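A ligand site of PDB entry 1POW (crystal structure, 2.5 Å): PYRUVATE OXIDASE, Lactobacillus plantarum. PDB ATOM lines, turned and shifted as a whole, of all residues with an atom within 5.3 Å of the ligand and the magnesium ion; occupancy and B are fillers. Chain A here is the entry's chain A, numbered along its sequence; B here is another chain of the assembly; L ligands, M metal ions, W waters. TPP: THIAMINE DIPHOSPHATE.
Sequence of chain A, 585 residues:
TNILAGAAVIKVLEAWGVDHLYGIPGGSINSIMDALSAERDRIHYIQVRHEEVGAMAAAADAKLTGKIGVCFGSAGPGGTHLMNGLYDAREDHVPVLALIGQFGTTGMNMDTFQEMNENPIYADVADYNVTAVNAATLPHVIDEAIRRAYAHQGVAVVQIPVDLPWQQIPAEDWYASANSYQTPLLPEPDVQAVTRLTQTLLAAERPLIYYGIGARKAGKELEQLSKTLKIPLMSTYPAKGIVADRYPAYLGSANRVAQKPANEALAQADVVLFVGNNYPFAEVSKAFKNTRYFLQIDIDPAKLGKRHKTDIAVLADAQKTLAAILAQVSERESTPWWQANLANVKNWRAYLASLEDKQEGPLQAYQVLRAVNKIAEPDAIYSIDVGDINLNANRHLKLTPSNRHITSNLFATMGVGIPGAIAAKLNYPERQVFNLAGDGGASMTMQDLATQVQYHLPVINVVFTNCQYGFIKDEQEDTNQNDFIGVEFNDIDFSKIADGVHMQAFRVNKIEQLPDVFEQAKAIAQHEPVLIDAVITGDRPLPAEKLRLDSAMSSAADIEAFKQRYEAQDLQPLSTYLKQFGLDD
Three residues have an atom within 4 Å of the magnesium ion: Asp 439, Asn 466 and Gln 468.
The nearest printed residue that does not touch the magnesium ion is Tyr 469 (4.1 Å).
The magnesium ion is bound by an oxygen (O3B) of the ligand, an oxygen (O1A) of the ligand, the backbone carbonyl oxygen of Gln 468, the side-chain carboxylate of Asp 439 and the side-chain amide oxygen of Asn 466.
Water W3 lies within hydrogen-bond range of an oxygen (O2B) of the ligand (2.7 Å), the backbone NH of Ile 389 (3.1 Å) and the backbone NH of Asp 388 (3.2 Å).
Water W1 lies within hydrogen-bond range of O of Val 386 (2.8 Å), O2A of the ligand (2.8 Å) and N of Gly 438 (3.0 Å).
O of Val 386 touches O2A of the ligand (3.9 Å).
CA of Gly 387 touches S1 of the ligand (3.9 Å).
Thr 413 touches the ligand (OG1 to CM2, 3.8 Å).
Met 414 touches the ligand (CE to O2A, 3.4 Å).
C of Gly 438 touches O2A of the ligand, 3.9 Å away.
Met 444 touches the ligand (SD to CM2, 3.99 Å).
Tyr 469 touches the ligand.
CD1 of Ile 472 touches C4 of the ligand, 3.6 Å away.
Ile 24 of chain B touches the ligand.
O of Pro 25 of chain B touches CM4 of the ligand, 3.5 Å away.
OG of Ser 74 of chain B touches C6' of the ligand, 3.4 Å away.
Pro 77 of chain B touches the ligand.
His 81 of chain B touches the ligand (ND1 to CM2, 3.5 Å).
Hydrophobic or aromatic side chains within 4 Å of the ligand: Met 414, Met 444, Tyr 469, Phe 471, Ile 472, Ile 24 of chain B, Pro 77 of chain B and His 81 of chain B.
Within 4 Å of the ligand: Val 386, Gly 387, Asp 388, Ala 412, Thr 413, Met 414, Gly 438, Asp 439, Gly 440, Gly 441, Met 444, Asn 466, Gln 468, Tyr 469, Gly 470, Phe 471, Ile 472, Ile 24 of chain B, Pro 25 of chain B, Glu 51 of chain B, Ser 74 of chain B, Pro 77 of chain B, His 81 of chain B and Gln 114 of chain B.
The nearest printed residue that does not touch the ligand is Gly 78 of chain B (4.01 Å).
A nitrogen (N1') of the ligand lies within hydrogen-bond range of the side-chain carboxylate (OE2) of Glu 51 of chain B (2.7 Å).
An oxygen (O1B) of the ligand is in hydrogen-bond range of the backbone NH of Gly 470, 3.1 Å away.
N of Gly 440 lies within hydrogen-bond range of O2A of the ligand (3.4 Å).
The backbone carbonyl oxygen (O) of Ala 412 is in hydrogen-bond range of a nitrogen (N4') of the ligand (2.8 Å).
O2A of the ligand sits at hydrogen-bond distance from N of Gly 441, at 2.9 Å.
An oxygen (O1B) of the ligand lies within hydrogen-bond range of the backbone NH of Phe 471 (2.9 Å).
The backbone NH of Asp 388 sits at hydrogen-bond distance from an oxygen (O1B) of the ligand, at 3.3 Å.
NE2 of Gln 114 of chain B lies close to N4' of the ligand (3.4 Å).
The backbone NH (N) of Asp 439 sits at hydrogen-bond distance from the backbone carbonyl oxygen (O) of Phe 464 (3.2 Å).
OD2 of Asp 439 is in hydrogen-bond range of N of Cys 467.
ND1 of His 81 of chain B is in hydrogen-bond range of OE1 of Glu 51 of chain B (2.8 Å).
O of Pro 77 of chain B lies within hydrogen-bond range of ND2 of Asn 84 (3.1 Å).
The side-chain amide nitrogen (NE2) of Gln 114 of chain B sits at hydrogen-bond distance from the backbone carbonyl oxygen (O) of Phe 411 (2.9 Å).
A ring nitrogen (NE2) of His 81 of chain B is in hydrogen-bond range of the side-chain amide nitrogen of Asn 84 (3.3 Å).
The side-chain hydroxyl of Thr 413 sits at hydrogen-bond distance from the side-chain amide nitrogen of Asn 84, 2.8 Å away.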
ATOM      1  N   ASN A  84     -27.091 -33.229  31.977  1.00  0.00           N
ATOM      2  CA  ASN A  84     -26.064 -32.246  32.282  1.00  0.00           C
ATOM      3  C   ASN A  84     -25.811 -32.110  33.755  1.00  0.00           C
ATOM      4  O   ASN A  84     -24.663 -31.941  34.156  1.00  0.00           O
ATOM      5  CB  ASN A  84     -26.440 -30.899  31.688  1.00  0.00           C
ATOM      6  CG  ASN A  84     -25.996 -30.812  30.231  1.00  0.00           C
ATOM      7  OD1 ASN A  84     -26.392 -31.598  29.365  1.00  0.00           O
ATOM      8  ND2 ASN A  84     -25.173 -29.861  29.805  1.00  0.00           N
ATOM      9  N   VAL A 386     -20.872 -20.231  33.663  1.00  0.00           N
ATOM     10  CA  VAL A 386     -19.629 -20.682  33.027  1.00  0.00           C
ATOM     11  C   VAL A 386     -19.455 -19.748  31.848  1.00  0.00           C
ATOM     12  O   VAL A 386     -20.428 -19.520  31.122  1.00  0.00           O
ATOM     13  CB  VAL A 386     -19.746 -22.145  32.552  1.00  0.00           C
ATOM     14  CG1 VAL A 386     -18.607 -22.543  31.629  1.00  0.00           C
ATOM     15  CG2 VAL A 386     -19.647 -23.064  33.747  1.00  0.00           C
ATOM     16  N   GLY A 387     -18.252 -19.229  31.675  1.00  0.00           N
ATOM     17  CA  GLY A 387     -17.984 -18.304  30.594  1.00  0.00           C
ATOM     18  C   GLY A 387     -17.029 -17.260  31.102  1.00  0.00           C
ATOM     19  O   GLY A 387     -16.232 -17.541  32.010  1.00  0.00           O
ATOM     20  N   ASP A 388     -17.062 -16.027  30.602  1.00  0.00           N
ATOM     21  CA  ASP A 388     -16.144 -15.009  31.073  1.00  0.00           C
ATOM     22  C   ASP A 388     -16.344 -14.717  32.539  1.00  0.00           C
ATOM     23  O   ASP A 388     -15.398 -14.313  33.223  1.00  0.00           O
ATOM     24  CB  ASP A 388     -16.318 -13.700  30.342  1.00  0.00           C
ATOM     25  CG  ASP A 388     -15.535 -13.512  29.045  1.00  0.00           C
ATOM     26  OD1 ASP A 388     -14.556 -14.229  28.789  1.00  0.00           O
ATOM     27  OD2 ASP A 388     -15.918 -12.610  28.300  1.00  0.00           O
ATOM     28  N   ILE A 389     -17.566 -14.944  33.064  1.00  0.00           N
ATOM     29  CA  ILE A 389     -17.843 -14.695  34.468  1.00  0.00           C
ATOM     30  C   ILE A 389     -16.936 -15.511  35.369  1.00  0.00           C
ATOM     31  O   ILE A 389     -16.643 -15.037  36.473  1.00  0.00           O
ATOM     32  CB  ILE A 389     -19.381 -14.971  34.761  1.00  0.00           C
ATOM     33  CG1 ILE A 389     -19.652 -14.557  36.208  1.00  0.00           C
ATOM     34  CG2 ILE A 389     -19.796 -16.420  34.557  1.00  0.00           C
ATOM     35  CD1 ILE A 389     -19.362 -13.083  36.591  1.00  0.00           C
ATOM     36  N   PHE A 411     -16.862 -30.285  33.994  1.00  0.00           N
ATOM     37  CA  PHE A 411     -17.768 -30.592  32.904  1.00  0.00           C
ATOM     38  C   PHE A 411     -18.088 -29.251  32.293  1.00  0.00           C
ATOM     39  O   PHE A 411     -18.292 -29.144  31.091  1.00  0.00           O
ATOM     40  CB  PHE A 411     -19.035 -31.239  33.435  1.00  0.00           C
ATOM     41  CG  PHE A 411     -19.928 -31.851  32.365  1.00  0.00           C
ATOM     42  CD1 PHE A 411     -19.409 -32.762  31.479  1.00  0.00           C
ATOM     43  CD2 PHE A 411     -21.261 -31.494  32.315  1.00  0.00           C
ATOM     44  CE1 PHE A 411     -20.232 -33.330  30.522  1.00  0.00           C
ATOM     45  CE2 PHE A 411     -22.079 -32.048  31.358  1.00  0.00           C
ATOM     46  CZ  PHE A 411     -21.556 -32.969  30.470  1.00  0.00           C
ATOM     47  N   ALA A 412     -18.173 -28.234  33.136  1.00  0.00           N
ATOM     48  CA  ALA A 412     -18.363 -26.851  32.751  1.00  0.00           C
ATOM     49  C   ALA A 412     -19.610 -26.588  31.930  1.00  0.00           C
ATOM     50  O   ALA A 412     -19.583 -25.997  30.852  1.00  0.00           O
ATOM     51  CB  ALA A 412     -17.144 -26.351  31.980  1.00  0.00           C
ATOM     52  N   THR A 413     -20.735 -27.037  32.478  1.00  0.00           N
ATOM     53  CA  THR A 413     -21.988 -26.790  31.819  1.00  0.00           C
ATOM     54  C   THR A 413     -22.487 -25.416  32.190  1.00  0.00           C
ATOM     55  O   THR A 413     -22.547 -24.978  33.349  1.00  0.00           O
ATOM     56  CB  THR A 413     -22.977 -27.914  32.212  1.00  0.00           C
ATOM     57  OG1 THR A 413     -24.092 -27.729  31.342  1.00  0.00           O
ATOM     58  CG2 THR A 413     -23.380 -27.949  33.665  1.00  0.00           C
ATOM     59  N   MET A 414     -22.858 -24.682  31.147  1.00  0.00           N
ATOM     60  CA  MET A 414     -23.548 -23.424  31.318  1.00  0.00           C
ATOM     61  C   MET A 414     -24.902 -23.836  31.866  1.00  0.00           C
ATOM     62  O   MET A 414     -25.279 -25.010  31.775  1.00  0.00           O
ATOM     63  CB  MET A 414     -23.741 -22.715  29.989  1.00  0.00           C
ATOM     64  CG  MET A 414     -22.467 -22.391  29.257  1.00  0.00           C
ATOM     65  SD  MET A 414     -22.837 -21.866  27.563  1.00  0.00           S
ATOM     66  CE  MET A 414     -23.610 -20.328  27.883  1.00  0.00           C
ATOM     67  N   GLY A 438     -23.646 -15.112  32.959  1.00  0.00           N
ATOM     68  CA  GLY A 438     -23.618 -14.405  31.702  1.00  0.00           C
ATOM     69  C   GLY A 438     -24.963 -14.644  31.043  1.00  0.00           C
ATOM     70  O   GLY A 438     -25.678 -15.604  31.394  1.00  0.00           O
ATOM     71  N   ASP A 439     -25.345 -13.791  30.105  1.00  0.00           N
ATOM     72  CA  ASP A 439     -26.561 -13.935  29.311  1.00  0.00           C
ATOM     73  C   ASP A 439     -26.764 -15.275  28.608  1.00  0.00           C
ATOM     74  O   ASP A 439     -27.903 -15.776  28.642  1.00  0.00           O
ATOM     75  CB  ASP A 439     -26.634 -12.828  28.249  1.00  0.00           C
ATOM     76  CG  ASP A 439     -25.443 -12.485  27.357  1.00  0.00           C
ATOM     77  OD1 ASP A 439     -24.378 -13.138  27.334  1.00  0.00           O
ATOM     78  OD2 ASP A 439     -25.556 -11.505  26.669  1.00  0.00           O
ATOM     79  N   GLY A 440     -25.744 -15.924  28.026  1.00  0.00           N
ATOM     80  CA  GLY A 440     -25.920 -17.198  27.342  1.00  0.00           C
ATOM     81  C   GLY A 440     -26.241 -18.286  28.355  1.00  0.00           C
ATOM     82  O   GLY A 440     -27.121 -19.123  28.185  1.00  0.00           O
ATOM     83  N   GLY A 441     -25.522 -18.256  29.473  1.00  0.00           N
ATOM     84  CA  GLY A 441     -25.730 -19.187  30.566  1.00  0.00           C
ATOM     85  C   GLY A 441     -27.083 -18.989  31.230  1.00  0.00           C
ATOM     86  O   GLY A 441     -27.767 -19.962  31.516  1.00  0.00           O
ATOM     87  N   ALA A 442     -27.487 -17.749  31.484  1.00  0.00           N
ATOM     88  CA  ALA A 442     -28.779 -17.461  32.082  1.00  0.00           C
ATOM     89  C   ALA A 442     -29.907 -17.806  31.130  1.00  0.00           C
ATOM     90  O   ALA A 442     -30.955 -18.247  31.608  1.00  0.00           O
ATOM     91  CB  ALA A 442     -28.886 -15.980  32.426  1.00  0.00           C
ATOM     92  N   MET A 444     -30.185 -20.367  29.015  1.00  0.00           N
ATOM     93  CA  MET A 444     -30.462 -21.792  29.036  1.00  0.00           C
ATOM     94  C   MET A 444     -31.297 -22.271  30.221  1.00  0.00           C
ATOM     95  O   MET A 444     -31.921 -23.327  30.114  1.00  0.00           O
ATOM     96  CB  MET A 444     -29.175 -22.599  29.041  1.00  0.00           C
ATOM     97  CG  MET A 444     -28.221 -22.281  27.927  1.00  0.00           C
ATOM     98  SD  MET A 444     -26.922 -23.537  27.828  1.00  0.00           S
ATOM     99  CE  MET A 444     -26.270 -23.099  26.252  1.00  0.00           C
ATOM    100  N   PHE A 464     -25.027 -10.675  33.198  1.00  0.00           N
ATOM    101  CA  PHE A 464     -24.033  -9.897  32.493  1.00  0.00           C
ATOM    102  C   PHE A 464     -24.353  -9.942  31.011  1.00  0.00           C
ATOM    103  O   PHE A 464     -23.955 -10.904  30.310  1.00  0.00           O
ATOM    104  CB  PHE A 464     -22.675 -10.505  32.767  1.00  0.00           C
ATOM    105  CG  PHE A 464     -22.154 -10.249  34.168  1.00  0.00           C
ATOM    106  CD1 PHE A 464     -22.665 -10.944  35.246  1.00  0.00           C
ATOM    107  CD2 PHE A 464     -21.180  -9.279  34.348  1.00  0.00           C
ATOM    108  CE1 PHE A 464     -22.182 -10.661  36.522  1.00  0.00           C
ATOM    109  CE2 PHE A 464     -20.710  -9.014  35.626  1.00  0.00           C
ATOM    110  CZ  PHE A 464     -21.212  -9.705  36.702  1.00  0.00           C
ATOM    111  N   ASN A 466     -23.887  -9.097  27.401  1.00  0.00           N
ATOM    112  CA  ASN A 466     -22.938  -8.648  26.401  1.00  0.00           C
ATOM    113  C   ASN A 466     -23.385  -8.991  24.998  1.00  0.00           C
ATOM    114  O   ASN A 466     -22.675  -8.680  24.057  1.00  0.00           O
ATOM    115  CB  ASN A 466     -21.543  -9.247  26.650  1.00  0.00           C
ATOM    116  CG  ASN A 466     -21.300 -10.743  26.833  1.00  0.00           C
ATOM    117  OD1 ASN A 466     -22.150 -11.662  26.870  1.00  0.00           O
ATOM    118  ND2 ASN A 466     -20.025 -11.069  26.983  1.00  0.00           N
ATOM    119  N   CYS A 467     -24.553  -9.629  24.801  1.00  0.00           N
ATOM    120  CA  CYS A 467     -25.092 -10.034  23.499  1.00  0.00           C
ATOM    121  C   CYS A 467     -24.114 -10.883  22.696  1.00  0.00           C
ATOM    122  O   CYS A 467     -24.056 -10.960  21.456  1.00  0.00           O
ATOM    123  CB  CYS A 467     -25.508  -8.798  22.686  1.00  0.00           C
ATOM    124  SG  CYS A 467     -26.813  -7.825  23.484  1.00  0.00           S
ATOM    125  N   GLN A 468     -23.395 -11.656  23.501  1.00  0.00           N
ATOM    126  CA  GLN A 468     -22.340 -12.518  23.020  1.00  0.00           C
ATOM    127  C   GLN A 468     -22.159 -13.667  23.987  1.00  0.00           C
ATOM    128  O   GLN A 468     -22.468 -13.627  25.208  1.00  0.00           O
ATOM    129  CB  GLN A 468     -20.986 -11.840  22.983  1.00  0.00           C
ATOM    130  CG  GLN A 468     -20.691 -10.665  22.097  1.00  0.00           C
ATOM    131  CD  GLN A 468     -19.354 -10.025  22.424  1.00  0.00           C
ATOM    132  OE1 GLN A 468     -19.184  -8.827  22.270  1.00  0.00           O
ATOM    133  NE2 GLN A 468     -18.296 -10.688  22.865  1.00  0.00           N
ATOM    134  N   TYR A 469     -21.500 -14.623  23.354  1.00  0.00           N
ATOM    135  CA  TYR A 469     -20.883 -15.762  23.992  1.00  0.00           C
ATOM    136  C   TYR A 469     -19.439 -15.243  23.979  1.00  0.00           C
ATOM    137  O   TYR A 469     -18.641 -15.593  23.101  1.00  0.00           O
ATOM    138  CB  TYR A 469     -21.021 -17.023  23.111  1.00  0.00           C
ATOM    139  CG  TYR A 469     -22.391 -17.668  23.061  1.00  0.00           C
ATOM    140  CD1 TYR A 469     -23.161 -17.826  24.205  1.00  0.00           C
ATOM    141  CD2 TYR A 469     -22.875 -18.099  21.842  1.00  0.00           C
ATOM    142  CE1 TYR A 469     -24.416 -18.415  24.131  1.00  0.00           C
ATOM    143  CE2 TYR A 469     -24.108 -18.689  21.755  1.00  0.00           C
ATOM    144  CZ  TYR A 469     -24.874 -18.833  22.899  1.00  0.00           C
ATOM    145  OH  TYR A 469     -26.135 -19.390  22.796  1.00  0.00           O
ATOM    146  N   GLY A 470     -19.073 -14.391  24.952  1.00  0.00           N
ATOM    147  CA  GLY A 470     -17.800 -13.690  24.976  1.00  0.00           C
ATOM    148  C   GLY A 470     -16.610 -14.656  25.030  1.00  0.00           C
ATOM    149  O   GLY A 470     -15.643 -14.494  24.253  1.00  0.00           O
ATOM    150  N   PHE A 471     -16.695 -15.697  25.872  1.00  0.00           N
ATOM    151  CA  PHE A 471     -15.610 -16.676  26.021  1.00  0.00           C
ATOM    152  C   PHE A 471     -15.255 -17.372  24.707  1.00  0.00           C
ATOM    153  O   PHE A 471     -14.078 -17.620  24.437  1.00  0.00           O
ATOM    154  CB  PHE A 471     -16.027 -17.721  27.057  1.00  0.00           C
ATOM    155  CG  PHE A 471     -14.893 -18.282  27.895  1.00  0.00           C
ATOM    156  CD1 PHE A 471     -14.113 -17.433  28.683  1.00  0.00           C
ATOM    157  CD2 PHE A 471     -14.629 -19.631  27.898  1.00  0.00           C
ATOM    158  CE1 PHE A 471     -13.085 -17.950  29.465  1.00  0.00           C
ATOM    159  CE2 PHE A 471     -13.597 -20.135  28.670  1.00  0.00           C
ATOM    160  CZ  PHE A 471     -12.822 -19.299  29.458  1.00  0.00           C
ATOM    161  N   ILE A 472     -16.252 -17.642  23.850  1.00  0.00           N
ATOM    162  CA  ILE A 472     -16.032 -18.304  22.565  1.00  0.00           C
ATOM    163  C   ILE A 472     -15.526 -17.306  21.536  1.00  0.00           C
ATOM    164  O   ILE A 472     -14.595 -17.626  20.772  1.00  0.00           O
ATOM    165  CB  ILE A 472     -17.341 -18.959  22.052  1.00  0.00           C
ATOM    166  CG1 ILE A 472     -17.922 -19.862  23.114  1.00  0.00           C
ATOM    167  CG2 ILE A 472     -17.060 -19.785  20.815  1.00  0.00           C
ATOM    168  CD1 ILE A 472     -16.942 -20.867  23.779  1.00  0.00           C
ATOM    169  N   PHE A 489     -25.278 -12.263  19.150  1.00  0.00           N
ATOM    170  CA  PHE A 489     -26.686 -12.550  18.983  1.00  0.00           C
ATOM    171  C   PHE A 489     -27.610 -11.450  19.462  1.00  0.00           C
ATOM    172  O   PHE A 489     -27.167 -10.426  19.985  1.00  0.00           O
ATOM    173  CB  PHE A 489     -27.014 -13.860  19.709  1.00  0.00           C
ATOM    174  CG  PHE A 489     -26.582 -13.983  21.173  1.00  0.00           C
ATOM    175  CD1 PHE A 489     -27.199 -13.260  22.168  1.00  0.00           C
ATOM    176  CD2 PHE A 489     -25.564 -14.874  21.493  1.00  0.00           C
ATOM    177  CE1 PHE A 489     -26.806 -13.410  23.485  1.00  0.00           C
ATOM    178  CE2 PHE A 489     -25.185 -15.020  22.802  1.00  0.00           C
ATOM    179  CZ  PHE A 489     -25.802 -14.296  23.797  1.00  0.00           C
ATOM    180  N   ILE B  24     -24.599 -24.488  18.830  1.00  0.00           N
ATOM    181  CA  ILE B  24     -24.002 -23.415  19.626  1.00  0.00           C
ATOM    182  C   ILE B  24     -22.506 -23.647  19.487  1.00  0.00           C
ATOM    183  O   ILE B  24     -22.094 -24.797  19.658  1.00  0.00           O
ATOM    184  CB  ILE B  24     -24.436 -23.513  21.132  1.00  0.00           C
ATOM    185  CG1 ILE B  24     -25.904 -23.165  21.230  1.00  0.00           C
ATOM    186  CG2 ILE B  24     -23.635 -22.564  22.031  1.00  0.00           C
ATOM    187  CD1 ILE B  24     -26.475 -23.231  22.644  1.00  0.00           C
ATOM    188  N   PRO B  25     -21.658 -22.650  19.171  1.00  0.00           N
ATOM    189  CA  PRO B  25     -20.229 -22.826  19.062  1.00  0.00           C
ATOM    190  C   PRO B  25     -19.569 -23.176  20.410  1.00  0.00           C
ATOM    191  O   PRO B  25     -20.168 -23.081  21.479  1.00  0.00           O
ATOM    192  CB  PRO B  25     -19.759 -21.505  18.459  1.00  0.00           C
ATOM    193  CG  PRO B  25     -20.731 -20.513  19.033  1.00  0.00           C
ATOM    194  CD  PRO B  25     -22.037 -21.265  18.901  1.00  0.00           C
ATOM    195  N   GLY B  26     -18.320 -23.573  20.340  1.00  0.00           N
ATOM    196  CA  GLY B  26     -17.528 -23.900  21.490  1.00  0.00           C
ATOM    197  C   GLY B  26     -16.126 -24.143  20.970  1.00  0.00           C
ATOM    198  O   GLY B  26     -15.939 -24.453  19.788  1.00  0.00           O
ATOM    199  N   GLU B  51     -28.956 -26.326  23.211  1.00  0.00           N
ATOM    200  CA  GLU B  51     -28.684 -27.354  22.212  1.00  0.00           C
ATOM    201  C   GLU B  51     -29.747 -28.414  21.960  1.00  0.00           C
ATOM    202  O   GLU B  51     -29.789 -28.971  20.863  1.00  0.00           O
ATOM    203  CB  GLU B  51     -27.403 -28.122  22.522  1.00  0.00           C
ATOM    204  CG  GLU B  51     -26.104 -27.326  22.484  1.00  0.00           C
ATOM    205  CD  GLU B  51     -25.644 -26.600  23.754  1.00  0.00           C
ATOM    206  OE1 GLU B  51     -26.381 -26.450  24.720  1.00  0.00           O
ATOM    207  OE2 GLU B  51     -24.507 -26.150  23.779  1.00  0.00           O
ATOM    208  N   SER B  74     -20.959 -28.843  21.276  1.00  0.00           N
ATOM    209  CA  SER B  74     -19.574 -28.909  21.701  1.00  0.00           C
ATOM    210  C   SER B  74     -19.358 -30.085  22.662  1.00  0.00           C
ATOM    211  O   SER B  74     -20.301 -30.760  23.090  1.00  0.00           O
ATOM    212  CB  SER B  74     -19.207 -27.577  22.352  1.00  0.00           C
ATOM    213  OG  SER B  74     -20.204 -27.088  23.240  1.00  0.00           O
ATOM    214  N   PRO B  77     -20.918 -30.910  27.847  1.00  0.00           N
ATOM    215  CA  PRO B  77     -22.266 -30.370  28.034  1.00  0.00           C
ATOM    216  C   PRO B  77     -23.064 -29.983  26.796  1.00  0.00           C
ATOM    217  O   PRO B  77     -24.304 -30.042  26.803  1.00  0.00           O
ATOM    218  CB  PRO B  77     -22.020 -29.220  29.000  1.00  0.00           C
ATOM    219  CG  PRO B  77     -20.627 -28.757  28.710  1.00  0.00           C
ATOM    220  CD  PRO B  77     -19.939 -30.096  28.577  1.00  0.00           C
ATOM    221  N   GLY B  78     -22.373 -29.570  25.718  1.00  0.00           N
ATOM    222  CA  GLY B  78     -23.026 -29.236  24.459  1.00  0.00           C
ATOM    223  C   GLY B  78     -23.686 -30.455  23.859  1.00  0.00           C
ATOM    224  O   GLY B  78     -24.846 -30.431  23.465  1.00  0.00           O
ATOM    225  N   HIS B  81     -26.681 -32.069  26.042  1.00  0.00           N
ATOM    226  CA  HIS B  81     -27.900 -31.314  25.835  1.00  0.00           C
ATOM    227  C   HIS B  81     -28.722 -31.781  24.629  1.00  0.00           C
ATOM    228  O   HIS B  81     -29.947 -31.621  24.610  1.00  0.00           O
ATOM    229  CB  HIS B  81     -27.576 -29.841  25.648  1.00  0.00           C
ATOM    230  CG  HIS B  81     -27.688 -28.993  26.894  1.00  0.00           C
ATOM    231  ND1 HIS B  81     -27.439 -27.704  27.035  1.00  0.00           N
ATOM    232  CD2 HIS B  81     -28.090 -29.438  28.115  1.00  0.00           C
ATOM    233  CE1 HIS B  81     -27.658 -27.359  28.272  1.00  0.00           C
ATOM    234  NE2 HIS B  81     -28.049 -28.414  28.912  1.00  0.00           N
ATOM    235  N   GLN B 114     -12.655 -30.441  30.118  1.00  0.00           N
ATOM    236  CA  GLN B 114     -13.826 -30.797  29.322  1.00  0.00           C
ATOM    237  C   GLN B 114     -13.578 -31.922  28.304  1.00  0.00           C
ATOM    238  O   GLN B 114     -14.266 -32.066  27.270  1.00  0.00           O
ATOM    239  CB  GLN B 114     -14.332 -29.504  28.643  1.00  0.00           C
ATOM    240  CG  GLN B 114     -15.774 -29.493  28.174  1.00  0.00           C
ATOM    241  CD  GLN B 114     -16.305 -28.075  27.976  1.00  0.00           C
ATOM    242  OE1 GLN B 114     -15.851 -27.294  27.130  1.00  0.00           O
ATOM    243  NE2 GLN B 114     -17.279 -27.679  28.777  1.00  0.00           N
HETATM  244  N1' TPP L   1     -22.955 -25.496  25.894  1.00  0.00           N
HETATM  245  C2' TPP L   1     -22.955 -25.859  27.166  1.00  0.00           C
HETATM  246  CM2 TPP L   1     -24.217 -26.476  27.768  1.00  0.00           C
HETATM  247  N3' TPP L   1     -21.876 -25.697  27.908  1.00  0.00           N
HETATM  248  C4' TPP L   1     -20.737 -25.199  27.390  1.00  0.00           C
HETATM  249  N4' TPP L   1     -19.615 -25.293  28.130  1.00  0.00           N
HETATM  250  C5' TPP L   1     -20.731 -24.719  26.070  1.00  0.00           C
HETATM  251  C6' TPP L   1     -21.861 -24.970  25.302  1.00  0.00           C
HETATM  252  C7' TPP L   1     -19.557 -23.929  25.423  1.00  0.00           C
HETATM  253  N3  TPP L   1     -19.351 -22.586  25.985  1.00  0.00           N
HETATM  254  C2  TPP L   1     -18.485 -22.410  26.956  1.00  0.00           C
HETATM  255  S1  TPP L   1     -18.394 -20.732  27.511  1.00  0.00           S
HETATM  256  C5  TPP L   1     -19.590 -20.376  26.262  1.00  0.00           C
HETATM  257  C4  TPP L   1     -19.980 -21.475  25.599  1.00  0.00           C
HETATM  258  CM4 TPP L   1     -21.015 -21.488  24.512  1.00  0.00           C
HETATM  259  C6  TPP L   1     -20.086 -18.971  26.028  1.00  0.00           C
HETATM  260  C7  TPP L   1     -20.495 -18.323  27.348  1.00  0.00           C
HETATM  261  O7  TPP L   1     -21.623 -17.353  27.074  1.00  0.00           O
HETATM  262  PA  TPP L   1     -22.228 -16.453  28.133  1.00  0.00           P
HETATM  263  O1A TPP L   1     -23.032 -15.443  27.465  1.00  0.00           O
HETATM  264  O2A TPP L   1     -22.865 -17.277  29.133  1.00  0.00           O
HETATM  265  O3A TPP L   1     -20.951 -15.679  28.764  1.00  0.00           O
HETATM  266  PB  TPP L   1     -19.924 -14.540  28.286  1.00  0.00           P
HETATM  267  O1B TPP L   1     -18.703 -15.212  27.899  1.00  0.00           O
HETATM  268  O2B TPP L   1     -19.771 -13.706  29.457  1.00  0.00           O
HETATM  269  O3B TPP L   1     -20.595 -13.842  27.200  1.00  0.00           O
HETATM  270 MG    MG M   1     -22.441 -13.617  27.192  1.00  0.00          MG
HETATM  271  O   HOH W   1     -22.204 -17.523  31.866  1.00  0.00           O
HETATM  272  O   HOH W   2     -19.352 -11.378  30.792  1.00  0.00           O
HETATM  273  O   HOH W   3     -20.108 -15.595  31.350  1.00  0.00           O
